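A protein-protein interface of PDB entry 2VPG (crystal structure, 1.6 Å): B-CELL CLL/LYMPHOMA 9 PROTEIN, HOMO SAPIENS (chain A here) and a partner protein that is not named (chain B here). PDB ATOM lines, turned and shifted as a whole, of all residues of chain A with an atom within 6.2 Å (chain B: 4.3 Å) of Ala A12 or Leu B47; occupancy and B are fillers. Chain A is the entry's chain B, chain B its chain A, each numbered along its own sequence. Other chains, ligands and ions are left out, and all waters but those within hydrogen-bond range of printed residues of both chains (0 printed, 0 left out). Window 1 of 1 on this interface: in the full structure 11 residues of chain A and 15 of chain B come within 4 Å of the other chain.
N of Met A11 sits at hydrogen-bond distance from OG of Ser A8 (3.1 Å).
Of chain A, only Phe A7 (3.7 Å) and Ala A12 (3.6 Å) come within 4 Å of Leu B47. Printed residues of chain A within 4 Å of Met B39: Thr A9 and Asn A13. Printed residues of chain B within 4 Å of Ala A15: Leu B46. Lys A14 touches none of the printed residues of chain B. Thr B48 touches none of the printed residues of chain A. The nearest printed residue of chain B that does not touch Ala A12 is Leu B46 (4.4 Å). The nearest residue of chain A that does not touch Leu B47 is Ser A8 (5.4 Å).
Of the 11 printed residues of chain B, 5 touch a printed residue of chain A. Hydrophobic or aromatic side chains of chain B that line the printed part of chain A: Met B39, Ala B43, Leu B46, Leu B47 and Trp B55. Along chain B the printed residues that touch a printed residue of chain A span positions 39 to 55. Of the 11 printed residues of chain A, 7 touch a printed residue of chain B. Hydrophobic or aromatic side chains of chain A within 4 Å of the printed part of chain B: Phe A7, Ala A12, Ala A15 and Ala A16. Along chain A the printed residues that touch a printed residue of chain B span positions 7 to 16.
Phe A7 touches Trp B55 (O to CA, 3.3 Å). Ser A8 touches Trp B55. N of Met B39 touches CG2 of Thr A9, at 3.7 Å. CB of Ala B43 touches O of Ala A12, 3.5 Å away. CD1 of Leu B47 touches CB of Ala A12, at 3.6 Å. OD1 of Asn A13 touches CA of Met B39 (3.5 Å). Asn A13 touches Ala B43 (OD1 to CB, 3.3 Å). Ala A15 touches Leu B46. Ala A16 touches Ala B43 (CB to N, 3.5 Å). Ala A16 touches Leu B46.
The side-chain hydroxyl (OG1) of Thr A9 sits at hydrogen-bond distance from the indole nitrogen (NE1) of Trp B55 (2.9 Å).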
ATOM      1  N   PHE A   7     -18.752   2.481  -2.919  1.00  0.00           N
ATOM      2  CA  PHE A   7     -20.011   2.841  -3.590  1.00  0.00           C
ATOM      3  C   PHE A   7     -21.056   1.725  -3.481  1.00  0.00           C
ATOM      4  O   PHE A   7     -20.762   0.548  -3.757  1.00  0.00           O
ATOM      5  CB  PHE A   7     -19.773   3.069  -5.084  1.00  0.00           C
ATOM      6  CG  PHE A   7     -18.983   4.303  -5.421  1.00  0.00           C
ATOM      7  CD1 PHE A   7     -19.626   5.432  -5.940  1.00  0.00           C
ATOM      8  CD2 PHE A   7     -17.590   4.320  -5.283  1.00  0.00           C
ATOM      9  CE1 PHE A   7     -18.895   6.580  -6.266  1.00  0.00           C
ATOM     10  CE2 PHE A   7     -16.852   5.450  -5.618  1.00  0.00           C
ATOM     11  CZ  PHE A   7     -17.506   6.586  -6.111  1.00  0.00           C
ATOM     12  N   SER A   8     -22.264   2.095  -3.078  1.00  0.00           N
ATOM     13  CA  SER A   8     -23.445   1.290  -3.346  1.00  0.00           C
ATOM     14  C   SER A   8     -23.824   1.468  -4.821  1.00  0.00           C
ATOM     15  O   SER A   8     -23.310   2.353  -5.508  1.00  0.00           O
ATOM     16  CB  SER A   8     -24.614   1.738  -2.478  1.00  0.00           C
ATOM     17  OG  SER A   8     -24.973   3.084  -2.818  1.00  0.00           O
ATOM     18  N   THR A   9     -24.741   0.633  -5.303  1.00  0.00           N
ATOM     19  CA  THR A   9     -25.272   0.801  -6.657  1.00  0.00           C
ATOM     20  C   THR A   9     -25.962   2.160  -6.818  1.00  0.00           C
ATOM     21  O   THR A   9     -25.753   2.857  -7.812  1.00  0.00           O
ATOM     22  CB  THR A   9     -26.275  -0.295  -6.998  1.00  0.00           C
ATOM     23  OG1 THR A   9     -25.641  -1.582  -6.874  1.00  0.00           O
ATOM     24  CG2 THR A   9     -26.776  -0.116  -8.419  1.00  0.00           C
ATOM     25  N   GLU A  10     -26.782   2.516  -5.839  1.00  0.00           N
ATOM     26  CA  GLU A  10     -27.480   3.793  -5.884  1.00  0.00           C
ATOM     27  C   GLU A  10     -26.497   4.952  -6.018  1.00  0.00           C
ATOM     28  O   GLU A  10     -26.672   5.815  -6.867  1.00  0.00           O
ATOM     29  CB  GLU A  10     -28.364   3.977  -4.655  1.00  0.00           C
ATOM     30  CG  GLU A  10     -28.775   5.447  -4.433  1.00  0.00           C
ATOM     31  CD  GLU A  10     -29.566   5.651  -3.157  1.00  0.00           C
ATOM     32  OE1 GLU A  10     -29.119   5.158  -2.095  1.00  0.00           O
ATOM     33  OE2 GLU A  10     -30.637   6.310  -3.216  1.00  0.00           O
ATOM     34  N   MET A  11     -25.453   4.952  -5.192  1.00  0.00           N
ATOM     35  CA  MET A  11     -24.429   5.994  -5.252  1.00  0.00           C
ATOM     36  C   MET A  11     -23.632   5.993  -6.555  1.00  0.00           C
ATOM     37  O   MET A  11     -23.285   7.047  -7.080  1.00  0.00           O
ATOM     38  CB  MET A  11     -23.488   5.895  -4.037  1.00  0.00           C
ATOM     39  CG  MET A  11     -24.165   6.209  -2.705  1.00  0.00           C
ATOM     40  SD  MET A  11     -24.956   7.847  -2.718  1.00  0.00           S
ATOM     41  CE  MET A  11     -23.594   8.832  -3.354  1.00  0.00           C
ATOM     42  N   ALA A  12     -23.349   4.808  -7.088  1.00  0.00           N
ATOM     43  CA  ALA A  12     -22.633   4.707  -8.353  1.00  0.00           C
ATOM     44  C   ALA A  12     -23.500   5.256  -9.497  1.00  0.00           C
ATOM     45  O   ALA A  12     -23.003   5.948 -10.383  1.00  0.00           O
ATOM     46  CB  ALA A  12     -22.242   3.259  -8.633  1.00  0.00           C
ATOM     47  N   ASN A  13     -24.796   4.939  -9.457  1.00  0.00           N
ATOM     48  CA  ASN A  13     -25.738   5.392 -10.492  1.00  0.00           C
ATOM     49  C   ASN A  13     -25.839   6.917 -10.498  1.00  0.00           C
ATOM     50  O   ASN A  13     -25.711   7.550 -11.547  1.00  0.00           O
ATOM     51  CB  ASN A  13     -27.120   4.749 -10.319  1.00  0.00           C
ATOM     52  CG  ASN A  13     -27.179   3.335 -10.872  1.00  0.00           C
ATOM     53  OD1 ASN A  13     -26.242   2.862 -11.517  1.00  0.00           O
ATOM     54  ND2 ASN A  13     -28.287   2.664 -10.630  1.00  0.00           N
ATOM     55  N   LYS A  14     -26.028   7.483  -9.309  1.00  0.00           N
ATOM     56  CA  LYS A  14     -26.060   8.939  -9.142  1.00  0.00           C
ATOM     57  C   LYS A  14     -24.753   9.608  -9.544  1.00  0.00           C
ATOM     58  O   LYS A  14     -24.764  10.612 -10.261  1.00  0.00           O
ATOM     59  CB  LYS A  14     -26.420   9.293  -7.704  1.00  0.00           C
ATOM     60  CG  LYS A  14     -27.865   9.025  -7.387  1.00  0.00           C
ATOM     61  CD  LYS A  14     -28.170   9.250  -5.927  1.00  0.00           C
ATOM     62  CE  LYS A  14     -29.671   9.208  -5.693  1.00  0.00           C
ATOM     63  NZ  LYS A  14     -30.012   9.048  -4.239  1.00  0.00           N
ATOM     64  N   ALA A  15     -23.628   9.051  -9.095  1.00  0.00           N
ATOM     65  CA  ALA A  15     -22.308   9.580  -9.432  1.00  0.00           C
ATOM     66  C   ALA A  15     -22.072   9.610 -10.933  1.00  0.00           C
ATOM     67  O   ALA A  15     -21.580  10.610 -11.468  1.00  0.00           O
ATOM     68  CB  ALA A  15     -21.199   8.774  -8.735  1.00  0.00           C
ATOM     69  N   ALA A  16     -22.440   8.514 -11.599  1.00  0.00           N
ATOM     70  CA  ALA A  16     -22.314   8.373 -13.045  1.00  0.00           C
ATOM     71  C   ALA A  16     -23.073   9.491 -13.772  1.00  0.00           C
ATOM     72  O   ALA A  16     -22.538  10.111 -14.680  1.00  0.00           O
ATOM     73  CB  ALA A  16     -22.859   7.017 -13.469  1.00  0.00           C
ATOM     74  N   GLU A  17     -24.311   9.743 -13.369  1.00  0.00           N
ATOM     75  CA  GLU A  17     -25.103  10.763 -14.052  1.00  0.00           C
ATOM     76  C   GLU A  17     -24.478  12.133 -13.832  1.00  0.00           C
ATOM     77  O   GLU A  17     -24.413  12.939 -14.765  1.00  0.00           O
ATOM     78  CB  GLU A  17     -26.568  10.736 -13.608  1.00  0.00           C
ATOM     79  CG  GLU A  17     -27.344   9.498 -14.098  1.00  0.00           C
ATOM     80  CD  GLU A  17     -27.122   9.162 -15.596  1.00  0.00           C
ATOM     81  OE1 GLU A  17     -27.317  10.046 -16.461  1.00  0.00           O
ATOM     82  OE2 GLU A  17     -26.770   7.993 -15.914  1.00  0.00           O
ATOM     83  N   ILE B  22     -19.808  -7.286 -11.674  1.00  0.00           N
ATOM     84  CA  ILE B  22     -18.971  -6.610 -10.671  1.00  0.00           C
ATOM     85  C   ILE B  22     -18.868  -7.470  -9.401  1.00  0.00           C
ATOM     86  O   ILE B  22     -19.824  -8.177  -9.011  1.00  0.00           O
ATOM     87  CB  ILE B  22     -19.504  -5.171 -10.399  1.00  0.00           C
ATOM     88  CG1 ILE B  22     -18.550  -4.383  -9.483  1.00  0.00           C
ATOM     89  CG2 ILE B  22     -20.927  -5.210  -9.881  1.00  0.00           C
ATOM     90  CD1 ILE B  22     -18.771  -2.859  -9.531  1.00  0.00           C
ATOM     91  N   MET B  39     -27.488  -1.587 -11.776  1.00  0.00           N
ATOM     92  CA  MET B  39     -26.443  -0.626 -12.128  1.00  0.00           C
ATOM     93  C   MET B  39     -26.504  -0.254 -13.608  1.00  0.00           C
ATOM     94  O   MET B  39     -26.661  -1.126 -14.458  1.00  0.00           O
ATOM     95  CB  MET B  39     -25.081  -1.227 -11.779  1.00  0.00           C
ATOM     96  CG  MET B  39     -23.899  -0.293 -11.979  1.00  0.00           C
ATOM     97  SD  MET B  39     -22.356  -1.143 -11.547  1.00  0.00           S
ATOM     98  CE  MET B  39     -22.641  -1.340  -9.803  1.00  0.00           C
ATOM     99  N   ALA B  43     -22.575   3.783 -14.826  1.00  0.00           N
ATOM    100  CA  ALA B  43     -22.047   3.548 -13.468  1.00  0.00           C
ATOM    101  C   ALA B  43     -21.014   2.419 -13.502  1.00  0.00           C
ATOM    102  O   ALA B  43     -19.965   2.486 -12.853  1.00  0.00           O
ATOM    103  CB  ALA B  43     -23.133   3.239 -12.522  1.00  0.00           C
ATOM    104  N   TYR B  44     -21.303   1.402 -14.318  1.00  0.00           N
ATOM    105  CA  TYR B  44     -20.438   0.230 -14.459  1.00  0.00           C
ATOM    106  C   TYR B  44     -19.083   0.627 -15.039  1.00  0.00           C
ATOM    107  O   TYR B  44     -18.034   0.249 -14.497  1.00  0.00           O
ATOM    108  CB  TYR B  44     -21.140  -0.813 -15.336  1.00  0.00           C
ATOM    109  CG  TYR B  44     -20.348  -2.091 -15.574  1.00  0.00           C
ATOM    110  CD1 TYR B  44     -20.241  -3.077 -14.576  1.00  0.00           C
ATOM    111  CD2 TYR B  44     -19.672  -2.300 -16.798  1.00  0.00           C
ATOM    112  CE1 TYR B  44     -19.508  -4.249 -14.815  1.00  0.00           C
ATOM    113  CE2 TYR B  44     -18.959  -3.450 -17.036  1.00  0.00           C
ATOM    114  CZ  TYR B  44     -18.856  -4.415 -16.036  1.00  0.00           C
ATOM    115  OH  TYR B  44     -18.143  -5.553 -16.305  1.00  0.00           O
ATOM    116  N   GLY B  45     -19.107   1.432 -16.108  1.00  0.00           N
ATOM    117  CA  GLY B  45     -17.888   1.964 -16.716  1.00  0.00           C
ATOM    118  C   GLY B  45     -17.118   2.856 -15.753  1.00  0.00           C
ATOM    119  O   GLY B  45     -15.882   2.780 -15.707  1.00  0.00           O
ATOM    120  N   LEU B  46     -17.840   3.664 -14.971  1.00  0.00           N
ATOM    121  CA  LEU B  46     -17.223   4.580 -13.985  1.00  0.00           C
ATOM    122  C   LEU B  46     -16.515   3.771 -12.896  1.00  0.00           C
ATOM    123  O   LEU B  46     -15.355   4.047 -12.554  1.00  0.00           O
ATOM    124  CB  LEU B  46     -18.276   5.506 -13.351  1.00  0.00           C
ATOM    125  CG  LEU B  46     -17.764   6.426 -12.232  1.00  0.00           C
ATOM    126  CD1 LEU B  46     -16.800   7.469 -12.796  1.00  0.00           C
ATOM    127  CD2 LEU B  46     -18.919   7.063 -11.464  1.00  0.00           C
ATOM    128  N   LEU B  47     -17.217   2.779 -12.355  1.00  0.00           N
ATOM    129  CA  LEU B  47     -16.639   1.933 -11.304  1.00  0.00           C
ATOM    130  C   LEU B  47     -15.433   1.161 -11.817  1.00  0.00           C
ATOM    131  O   LEU B  47     -14.430   1.024 -11.094  1.00  0.00           O
ATOM    132  CB  LEU B  47     -17.706   1.026 -10.666  1.00  0.00           C
ATOM    133  CG  LEU B  47     -18.728   1.704  -9.734  1.00  0.00           C
ATOM    134  CD1 LEU B  47     -19.814   0.742  -9.333  1.00  0.00           C
ATOM    135  CD2 LEU B  47     -18.115   2.322  -8.467  1.00  0.00           C
ATOM    136  N   THR B  48     -15.491   0.705 -13.068  1.00  0.00           N
ATOM    137  CA  THR B  48     -14.346   0.045 -13.703  1.00  0.00           C
ATOM    138  C   THR B  48     -13.125   0.980 -13.759  1.00  0.00           C
ATOM    139  O   THR B  48     -12.001   0.574 -13.436  1.00  0.00           O
ATOM    140  CB  THR B  48     -14.687  -0.456 -15.131  1.00  0.00           C
ATOM    141  OG1 THR B  48     -15.760  -1.405 -15.074  1.00  0.00           O
ATOM    142  CG2 THR B  48     -13.480  -1.134 -15.792  1.00  0.00           C
ATOM    143  N   ALA B  49     -13.375   2.228 -14.151  1.00  0.00           N
ATOM    144  CA  ALA B  49     -12.326   3.235 -14.367  1.00  0.00           C
ATOM    145  C   ALA B  49     -11.700   3.764 -13.072  1.00  0.00           C
ATOM    146  O   ALA B  49     -10.565   4.279 -13.091  1.00  0.00           O
ATOM    147  CB  ALA B  49     -12.894   4.401 -15.181  1.00  0.00           C
ATOM    148  N   GLU B  50     -12.445   3.659 -11.973  1.00  0.00           N
ATOM    149  CA  GLU B  50     -12.015   4.116 -10.660  1.00  0.00           C
ATOM    150  C   GLU B  50     -11.153   3.074  -9.935  1.00  0.00           C
ATOM    151  O   GLU B  50     -11.679   2.240  -9.180  1.00  0.00           O
ATOM    152  CB  GLU B  50     -13.233   4.457  -9.794  1.00  0.00           C
ATOM    153  CG  GLU B  50     -14.034   5.694 -10.230  1.00  0.00           C
ATOM    154  CD  GLU B  50     -13.278   7.002 -10.023  1.00  0.00           C
ATOM    155  OE1 GLU B  50     -12.560   7.137  -9.006  1.00  0.00           O
ATOM    156  OE2 GLU B  50     -13.393   7.888 -10.892  1.00  0.00           O
ATOM    157  N   TRP B  55     -17.117  -1.568  -4.897  1.00  0.00           N
ATOM    158  CA  TRP B  55     -18.550  -1.638  -4.854  1.00  0.00           C
ATOM    159  C   TRP B  55     -18.991  -2.662  -3.812  1.00  0.00           C
ATOM    160  O   TRP B  55     -18.330  -3.698  -3.597  1.00  0.00           O
ATOM    161  CB  TRP B  55     -19.076  -1.983  -6.265  1.00  0.00           C
ATOM    162  CG  TRP B  55     -20.545  -2.275  -6.333  1.00  0.00           C
ATOM    163  CD1 TRP B  55     -21.562  -1.358  -6.411  1.00  0.00           C
ATOM    164  CD2 TRP B  55     -21.171  -3.569  -6.334  1.00  0.00           C
ATOM    165  NE1 TRP B  55     -22.776  -2.004  -6.449  1.00  0.00           N
ATOM    166  CE2 TRP B  55     -22.568  -3.358  -6.400  1.00  0.00           C
ATOM    167  CE3 TRP B  55     -20.690  -4.883  -6.254  1.00  0.00           C
ATOM    168  CZ2 TRP B  55     -23.495  -4.411  -6.427  1.00  0.00           C
ATOM    169  CZ3 TRP B  55     -21.632  -5.954  -6.288  1.00  0.00           C
ATOM    170  CH2 TRP B  55     -23.008  -5.699  -6.357  1.00  0.00           C
